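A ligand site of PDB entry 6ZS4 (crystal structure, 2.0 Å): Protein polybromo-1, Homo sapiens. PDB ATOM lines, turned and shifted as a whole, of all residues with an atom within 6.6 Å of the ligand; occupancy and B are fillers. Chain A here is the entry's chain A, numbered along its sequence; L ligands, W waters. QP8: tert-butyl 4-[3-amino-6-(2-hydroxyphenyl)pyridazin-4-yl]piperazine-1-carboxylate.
O of Ile 41 touches C4 of the ligand, 3.3 Å away. Phe 42 touches the ligand. CD1 of Leu 45 touches C4 of the ligand, at 3.7 Å. Pro 46 touches the ligand (CG to C10, 3.9 Å). Leu 51 touches the ligand. Met 62 touches the ligand (O to C, 3.2 Å). Asp 63 touches the ligand (CB to C5, 3.99 Å). Met 89 touches the ligand. Ala 93 touches the ligand (CA to O2, 3.3 Å). CE2 of Tyr 96 touches N4 of the ligand, at 3.6 Å. Ile 103 touches the ligand (CD1 to N4, 3.5 Å). The nearest printed residue that does not touch the ligand is Glu 50 (4.03 Å).
An oxygen (O2) of the ligand sits at hydrogen-bond distance from the side-chain hydroxyl of Tyr 54, at 2.8 Å. A nitrogen (N1) of the ligand is in hydrogen-bond range of the side-chain amide nitrogen (ND2) of Asn 97, at 3.1 Å.
The side-chain carboxylate of Asp 63 lies within hydrogen-bond range of the backbone NH of Leu 45, at 2.9 Å. ND2 of Asn 97 sits at hydrogen-bond distance from O of Ala 93 (2.8 Å). N of Met 64 is in hydrogen-bond range of O of Phe 42.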
ATOM      1  N   ILE A  41     -17.116 -25.562 -12.098  1.00  0.00           N
ATOM      2  CA  ILE A  41     -15.755 -25.261 -12.508  1.00  0.00           C
ATOM      3  C   ILE A  41     -15.056 -24.283 -11.565  1.00  0.00           C
ATOM      4  O   ILE A  41     -13.818 -24.264 -11.507  1.00  0.00           O
ATOM      5  CB  ILE A  41     -15.744 -24.737 -13.967  1.00  0.00           C
ATOM      6  CG1 ILE A  41     -14.311 -24.686 -14.522  1.00  0.00           C
ATOM      7  CG2 ILE A  41     -16.399 -23.375 -14.056  1.00  0.00           C
ATOM      8  CD1 ILE A  41     -13.647 -26.053 -14.554  1.00  0.00           C
ATOM      9  N   PHE A  42     -15.791 -23.483 -10.784  1.00  0.00           N
ATOM     10  CA  PHE A  42     -15.221 -22.402  -9.996  1.00  0.00           C
ATOM     11  C   PHE A  42     -14.968 -22.767  -8.542  1.00  0.00           C
ATOM     12  O   PHE A  42     -14.433 -21.941  -7.786  1.00  0.00           O
ATOM     13  CB  PHE A  42     -16.124 -21.158 -10.062  1.00  0.00           C
ATOM     14  CG  PHE A  42     -16.394 -20.686 -11.460  1.00  0.00           C
ATOM     15  CD1 PHE A  42     -15.368 -20.188 -12.243  1.00  0.00           C
ATOM     16  CD2 PHE A  42     -17.657 -20.753 -12.000  1.00  0.00           C
ATOM     17  CE1 PHE A  42     -15.602 -19.756 -13.536  1.00  0.00           C
ATOM     18  CE2 PHE A  42     -17.911 -20.313 -13.281  1.00  0.00           C
ATOM     19  CZ  PHE A  42     -16.874 -19.823 -14.065  1.00  0.00           C
ATOM     20  N   LEU A  43     -15.305 -23.995  -8.132  1.00  0.00           N
ATOM     21  CA  LEU A  43     -15.062 -24.419  -6.749  1.00  0.00           C
ATOM     22  C   LEU A  43     -13.579 -24.413  -6.395  1.00  0.00           C
ATOM     23  O   LEU A  43     -13.173 -23.831  -5.379  1.00  0.00           O
ATOM     24  CB  LEU A  43     -15.653 -25.808  -6.516  1.00  0.00           C
ATOM     25  CG  LEU A  43     -17.162 -25.921  -6.749  1.00  0.00           C
ATOM     26  CD1 LEU A  43     -17.681 -27.245  -6.150  1.00  0.00           C
ATOM     27  CD2 LEU A  43     -17.871 -24.719  -6.162  1.00  0.00           C
ATOM     28  N   ARG A  44     -12.752 -25.072  -7.203  1.00  0.00           N
ATOM     29  CA  ARG A  44     -11.353 -25.278  -6.815  1.00  0.00           C
ATOM     30  C   ARG A  44     -10.459 -24.980  -8.011  1.00  0.00           C
ATOM     31  O   ARG A  44     -10.460 -25.721  -8.993  1.00  0.00           O
ATOM     32  CB  ARG A  44     -11.103 -26.697  -6.311  1.00  0.00           C
ATOM     33  CG  ARG A  44      -9.749 -26.848  -5.615  1.00  0.00           C
ATOM     34  CD  ARG A  44      -9.449 -28.288  -5.237  1.00  0.00           C
ATOM     35  NE  ARG A  44     -10.382 -28.774  -4.232  1.00  0.00           N
ATOM     36  CZ  ARG A  44     -10.517 -30.049  -3.875  1.00  0.00           C
ATOM     37  NH1 ARG A  44      -9.767 -30.985  -4.459  1.00  0.00           N
ATOM     38  NH2 ARG A  44     -11.404 -30.397  -2.952  1.00  0.00           N
ATOM     39  N   LEU A  45      -9.698 -23.896  -7.907  1.00  0.00           N
ATOM     40  CA  LEU A  45      -8.706 -23.584  -8.922  1.00  0.00           C
ATOM     41  C   LEU A  45      -7.521 -24.530  -8.749  1.00  0.00           C
ATOM     42  O   LEU A  45      -7.075 -24.753  -7.625  1.00  0.00           O
ATOM     43  CB  LEU A  45      -8.265 -22.143  -8.796  1.00  0.00           C
ATOM     44  CG  LEU A  45      -7.191 -21.622  -9.764  1.00  0.00           C
ATOM     45  CD1 LEU A  45      -7.750 -21.544 -11.161  1.00  0.00           C
ATOM     46  CD2 LEU A  45      -6.735 -20.252  -9.279  1.00  0.00           C
ATOM     47  N   PRO A  46      -7.011 -25.133  -9.823  1.00  0.00           N
ATOM     48  CA  PRO A  46      -5.820 -25.987  -9.689  1.00  0.00           C
ATOM     49  C   PRO A  46      -4.649 -25.185  -9.153  1.00  0.00           C
ATOM     50  O   PRO A  46      -4.570 -23.973  -9.345  1.00  0.00           O
ATOM     51  CB  PRO A  46      -5.563 -26.473 -11.126  1.00  0.00           C
ATOM     52  CG  PRO A  46      -6.919 -26.322 -11.832  1.00  0.00           C
ATOM     53  CD  PRO A  46      -7.524 -25.100 -11.206  1.00  0.00           C
ATOM     54  N   GLU A  50       0.017 -27.466 -10.853  1.00  0.00           N
ATOM     55  CA  GLU A  50      -0.759 -28.117 -11.901  1.00  0.00           C
ATOM     56  C   GLU A  50      -0.986 -27.175 -13.072  1.00  0.00           C
ATOM     57  O   GLU A  50      -0.998 -27.620 -14.228  1.00  0.00           O
ATOM     58  CB  GLU A  50      -2.088 -28.621 -11.307  1.00  0.00           C
ATOM     59  CG  GLU A  50      -1.889 -29.479 -10.030  1.00  0.00           C
ATOM     60  CD  GLU A  50      -3.172 -29.715  -9.193  1.00  0.00           C
ATOM     61  OE1 GLU A  50      -3.878 -28.737  -8.823  1.00  0.00           O
ATOM     62  OE2 GLU A  50      -3.466 -30.894  -8.907  1.00  0.00           O
ATOM     63  N   LEU A  51      -1.104 -25.868 -12.819  1.00  0.00           N
ATOM     64  CA  LEU A  51      -1.597 -24.921 -13.821  1.00  0.00           C
ATOM     65  C   LEU A  51      -0.781 -23.638 -13.758  1.00  0.00           C
ATOM     66  O   LEU A  51      -1.287 -22.567 -13.398  1.00  0.00           O
ATOM     67  CB  LEU A  51      -3.091 -24.645 -13.593  1.00  0.00           C
ATOM     68  CG  LEU A  51      -3.881 -23.918 -14.669  1.00  0.00           C
ATOM     69  CD1 LEU A  51      -4.023 -24.787 -15.881  1.00  0.00           C
ATOM     70  CD2 LEU A  51      -5.262 -23.512 -14.099  1.00  0.00           C
ATOM     71  N   TYR A  54      -1.922 -20.085 -15.587  1.00  0.00           N
ATOM     72  CA  TYR A  54      -3.012 -19.295 -15.019  1.00  0.00           C
ATOM     73  C   TYR A  54      -2.506 -18.268 -14.034  1.00  0.00           C
ATOM     74  O   TYR A  54      -3.018 -17.148 -13.974  1.00  0.00           O
ATOM     75  CB  TYR A  54      -4.022 -20.202 -14.318  1.00  0.00           C
ATOM     76  CG  TYR A  54      -5.289 -19.519 -13.814  1.00  0.00           C
ATOM     77  CD1 TYR A  54      -5.310 -18.818 -12.609  1.00  0.00           C
ATOM     78  CD2 TYR A  54      -6.478 -19.602 -14.533  1.00  0.00           C
ATOM     79  CE1 TYR A  54      -6.483 -18.195 -12.136  1.00  0.00           C
ATOM     80  CE2 TYR A  54      -7.661 -18.979 -14.070  1.00  0.00           C
ATOM     81  CZ  TYR A  54      -7.662 -18.286 -12.867  1.00  0.00           C
ATOM     82  OH  TYR A  54      -8.845 -17.674 -12.404  1.00  0.00           O
ATOM     83  N   ILE A  58      -3.114 -14.060 -14.235  1.00  0.00           N
ATOM     84  CA  ILE A  58      -4.075 -13.654 -13.227  1.00  0.00           C
ATOM     85  C   ILE A  58      -3.330 -13.112 -12.017  1.00  0.00           C
ATOM     86  O   ILE A  58      -2.610 -13.863 -11.347  1.00  0.00           O
ATOM     87  CB  ILE A  58      -4.985 -14.822 -12.814  1.00  0.00           C
ATOM     88  CG1 ILE A  58      -5.980 -15.111 -13.931  1.00  0.00           C
ATOM     89  CG2 ILE A  58      -5.669 -14.517 -11.496  1.00  0.00           C
ATOM     90  CD1 ILE A  58      -6.634 -13.854 -14.496  1.00  0.00           C
ATOM     91  N   MET A  62      -8.552 -16.692  -7.232  1.00  0.00           N
ATOM     92  CA  MET A  62      -9.693 -16.775  -6.337  1.00  0.00           C
ATOM     93  C   MET A  62     -10.571 -17.940  -6.772  1.00  0.00           C
ATOM     94  O   MET A  62     -10.742 -18.169  -7.966  1.00  0.00           O
ATOM     95  CB  MET A  62     -10.469 -15.448  -6.354  1.00  0.00           C
ATOM     96  CG  MET A  62     -11.692 -15.419  -5.447  1.00  0.00           C
ATOM     97  SD  MET A  62     -11.282 -15.536  -3.693  1.00  0.00           S
ATOM     98  CE  MET A  62      -9.935 -14.349  -3.580  1.00  0.00           C
ATOM     99  N   ASP A  63     -11.126 -18.677  -5.804  1.00  0.00           N
ATOM    100  CA  ASP A  63     -12.132 -19.679  -6.131  1.00  0.00           C
ATOM    101  C   ASP A  63     -13.173 -19.737  -5.024  1.00  0.00           C
ATOM    102  O   ASP A  63     -13.018 -19.123  -3.961  1.00  0.00           O
ATOM    103  CB  ASP A  63     -11.531 -21.065  -6.388  1.00  0.00           C
ATOM    104  CG  ASP A  63     -10.740 -21.604  -5.208  1.00  0.00           C
ATOM    105  OD1 ASP A  63     -11.061 -21.276  -4.059  1.00  0.00           O
ATOM    106  OD2 ASP A  63      -9.790 -22.380  -5.448  1.00  0.00           O
ATOM    107  N   MET A  64     -14.236 -20.507  -5.260  1.00  0.00           N
ATOM    108  CA  MET A  64     -15.358 -20.458  -4.333  1.00  0.00           C
ATOM    109  C   MET A  64     -15.003 -21.119  -2.998  1.00  0.00           C
ATOM    110  O   MET A  64     -15.487 -20.684  -1.950  1.00  0.00           O
ATOM    111  CB  MET A  64     -16.573 -21.078  -5.002  1.00  0.00           C
ATOM    112  CG  MET A  64     -16.980 -20.294  -6.228  1.00  0.00           C
ATOM    113  SD  MET A  64     -18.621 -20.709  -6.876  1.00  0.00           S
ATOM    114  CE  MET A  64     -19.611 -20.494  -5.386  1.00  0.00           C
ATOM    115  N   MET A  89     -13.186 -13.220  -9.080  1.00  0.00           N
ATOM    116  CA  MET A  89     -13.101 -14.581  -9.613  1.00  0.00           C
ATOM    117  C   MET A  89     -13.657 -14.643 -11.023  1.00  0.00           C
ATOM    118  O   MET A  89     -13.071 -15.285 -11.896  1.00  0.00           O
ATOM    119  CB  MET A  89     -13.870 -15.540  -8.697  1.00  0.00           C
ATOM    120  CG  MET A  89     -13.777 -16.994  -9.142  1.00  0.00           C
ATOM    121  SD  MET A  89     -14.807 -18.007  -8.069  1.00  0.00           S
ATOM    122  CE  MET A  89     -16.439 -17.676  -8.721  1.00  0.00           C
ATOM    123  N   PHE A  90     -14.795 -14.002 -11.259  1.00  0.00           N
ATOM    124  CA  PHE A  90     -15.408 -14.102 -12.583  1.00  0.00           C
ATOM    125  C   PHE A  90     -14.613 -13.308 -13.616  1.00  0.00           C
ATOM    126  O   PHE A  90     -14.520 -13.701 -14.782  1.00  0.00           O
ATOM    127  CB  PHE A  90     -16.853 -13.624 -12.548  1.00  0.00           C
ATOM    128  CG  PHE A  90     -17.782 -14.506 -11.724  1.00  0.00           C
ATOM    129  CD1 PHE A  90     -17.800 -15.891 -11.904  1.00  0.00           C
ATOM    130  CD2 PHE A  90     -18.637 -13.945 -10.794  1.00  0.00           C
ATOM    131  CE1 PHE A  90     -18.674 -16.694 -11.155  1.00  0.00           C
ATOM    132  CE2 PHE A  90     -19.511 -14.739 -10.034  1.00  0.00           C
ATOM    133  CZ  PHE A  90     -19.520 -16.112 -10.216  1.00  0.00           C
ATOM    134  N   ASN A  92     -11.454 -12.986 -13.445  1.00  0.00           N
ATOM    135  CA  ASN A  92     -10.302 -13.851 -13.690  1.00  0.00           C
ATOM    136  C   ASN A  92     -10.615 -14.874 -14.766  1.00  0.00           C
ATOM    137  O   ASN A  92      -9.872 -15.022 -15.744  1.00  0.00           O
ATOM    138  CB  ASN A  92      -9.856 -14.552 -12.395  1.00  0.00           C
ATOM    139  CG  ASN A  92      -9.141 -13.603 -11.424  1.00  0.00           C
ATOM    140  OD1 ASN A  92      -8.765 -12.494 -11.782  1.00  0.00           O
ATOM    141  ND2 ASN A  92      -8.960 -14.059 -10.177  1.00  0.00           N
ATOM    142  N   ALA A  93     -11.745 -15.583 -14.610  1.00  0.00           N
ATOM    143  CA  ALA A  93     -12.144 -16.568 -15.596  1.00  0.00           C
ATOM    144  C   ALA A  93     -12.287 -15.953 -16.985  1.00  0.00           C
ATOM    145  O   ALA A  93     -11.957 -16.588 -17.980  1.00  0.00           O
ATOM    146  CB  ALA A  93     -13.464 -17.237 -15.188  1.00  0.00           C
ATOM    147  N   CYS A  94     -12.855 -14.732 -17.067  1.00  0.00           N
ATOM    148  CA  CYS A  94     -13.031 -14.093 -18.362  1.00  0.00           C
ATOM    149  C   CYS A  94     -11.729 -13.502 -18.921  1.00  0.00           C
ATOM    150  O   CYS A  94     -11.705 -13.068 -20.070  1.00  0.00           O
ATOM    151  CB  CYS A  94     -14.072 -12.990 -18.255  1.00  0.00           C
ATOM    152  SG  CYS A  94     -15.715 -13.718 -17.994  1.00  0.00           S
ATOM    153  N   TYR A  96      -8.775 -15.485 -18.498  1.00  0.00           N
ATOM    154  CA  TYR A  96      -7.978 -16.645 -18.872  1.00  0.00           C
ATOM    155  C   TYR A  96      -8.568 -17.382 -20.063  1.00  0.00           C
ATOM    156  O   TYR A  96      -7.823 -17.877 -20.909  1.00  0.00           O
ATOM    157  CB  TYR A  96      -7.839 -17.567 -17.650  1.00  0.00           C
ATOM    158  CG  TYR A  96      -7.027 -18.821 -17.887  1.00  0.00           C
ATOM    159  CD1 TYR A  96      -5.631 -18.784 -17.845  1.00  0.00           C
ATOM    160  CD2 TYR A  96      -7.646 -20.036 -18.120  1.00  0.00           C
ATOM    161  CE1 TYR A  96      -4.888 -19.925 -18.041  1.00  0.00           C
ATOM    162  CE2 TYR A  96      -6.902 -21.198 -18.327  1.00  0.00           C
ATOM    163  CZ  TYR A  96      -5.520 -21.122 -18.282  1.00  0.00           C
ATOM    164  OH  TYR A  96      -4.768 -22.252 -18.479  1.00  0.00           O
ATOM    165  N   ASN A  97      -9.909 -17.440 -20.182  1.00  0.00           N
ATOM    166  CA  ASN A  97     -10.592 -18.079 -21.290  1.00  0.00           C
ATOM    167  C   ASN A  97     -11.144 -17.057 -22.294  1.00  0.00           C
ATOM    168  O   ASN A  97     -11.473 -15.928 -21.931  1.00  0.00           O
ATOM    169  CB  ASN A  97     -11.757 -18.946 -20.772  1.00  0.00           C
ATOM    170  CG  ASN A  97     -11.344 -19.857 -19.630  1.00  0.00           C
ATOM    171  OD1 ASN A  97     -10.957 -21.005 -19.848  1.00  0.00           O
ATOM    172  ND2 ASN A  97     -11.423 -19.354 -18.403  1.00  0.00           N
ATOM    173  N   ILE A 103     -16.608 -21.716 -20.274  1.00  0.00           N
ATOM    174  CA  ILE A 103     -16.272 -21.202 -18.940  1.00  0.00           C
ATOM    175  C   ILE A 103     -16.483 -19.687 -18.873  1.00  0.00           C
ATOM    176  O   ILE A 103     -16.991 -19.172 -17.871  1.00  0.00           O
ATOM    177  CB  ILE A 103     -14.846 -21.647 -18.550  1.00  0.00           C
ATOM    178  CG1 ILE A 103     -14.835 -23.163 -18.304  1.00  0.00           C
ATOM    179  CG2 ILE A 103     -14.315 -20.888 -17.312  1.00  0.00           C
ATOM    180  CD1 ILE A 103     -13.451 -23.732 -17.952  1.00  0.00           C
HETATM  181  C4  QP8 L   1     -11.442 -21.935 -11.568  1.00  0.00           C
HETATM  182  C5  QP8 L   1     -11.800 -21.390 -10.360  1.00  0.00           C
HETATM  183  C6  QP8 L   1     -10.808 -21.734 -13.986  1.00  0.00           C
HETATM  184  N1  QP8 L   1     -10.570 -21.378 -16.267  1.00  0.00           N
HETATM  185  C7  QP8 L   1     -10.167 -22.637 -16.449  1.00  0.00           C
HETATM  186  C8  QP8 L   1     -10.025 -23.515 -15.348  1.00  0.00           C
HETATM  187  N2  QP8 L   1      -9.474 -24.787 -15.577  1.00  0.00           N
HETATM  188  C9  QP8 L   1     -10.369 -23.052 -14.083  1.00  0.00           C
HETATM  189  C10 QP8 L   1      -9.628 -25.775 -14.516  1.00  0.00           C
HETATM  190  C11 QP8 L   1      -9.369 -27.168 -15.059  1.00  0.00           C
HETATM  191  C12 QP8 L   1      -7.778 -26.168 -16.676  1.00  0.00           C
HETATM  192  N3  QP8 L   1      -8.043 -27.236 -15.706  1.00  0.00           N
HETATM  193  C13 QP8 L   1      -8.085 -24.813 -16.059  1.00  0.00           C
HETATM  194  C14 QP8 L   1      -7.248 -28.304 -15.514  1.00  0.00           C
HETATM  195  C15 QP8 L   1      -5.065 -29.234 -16.222  1.00  0.00           C
HETATM  196  N4  QP8 L   1     -10.007 -23.019 -17.733  1.00  0.00           N
HETATM  197  O   QP8 L   1      -7.514 -29.204 -14.761  1.00  0.00           O
HETATM  198  O1  QP8 L   1      -6.123 -28.189 -16.246  1.00  0.00           O
HETATM  199  C18 QP8 L   1      -4.575 -29.382 -14.799  1.00  0.00           C
HETATM  200  C17 QP8 L   1      -3.963 -28.723 -17.134  1.00  0.00           C
HETATM  201  C16 QP8 L   1      -5.645 -30.526 -16.753  1.00  0.00           C
HETATM  202  N   QP8 L   1     -10.886 -20.931 -15.046  1.00  0.00           N
HETATM  203  C3  QP8 L   1     -11.193 -21.125 -12.683  1.00  0.00           C
HETATM  204  C2  QP8 L   1     -11.330 -19.736 -12.526  1.00  0.00           C
HETATM  205  O2  QP8 L   1     -11.067 -18.898 -13.571  1.00  0.00           O
HETATM  206  C1  QP8 L   1     -11.696 -19.194 -11.297  1.00  0.00           C
HETATM  207  C   QP8 L   1     -11.937 -20.021 -10.224  1.00  0.00           C
HETATM  208  O   HOH W   1      -1.257 -30.227 -14.722  1.00  0.00           O
HETATM  209  O   HOH W   2      -0.882 -27.229 -16.767  1.00  0.00           O
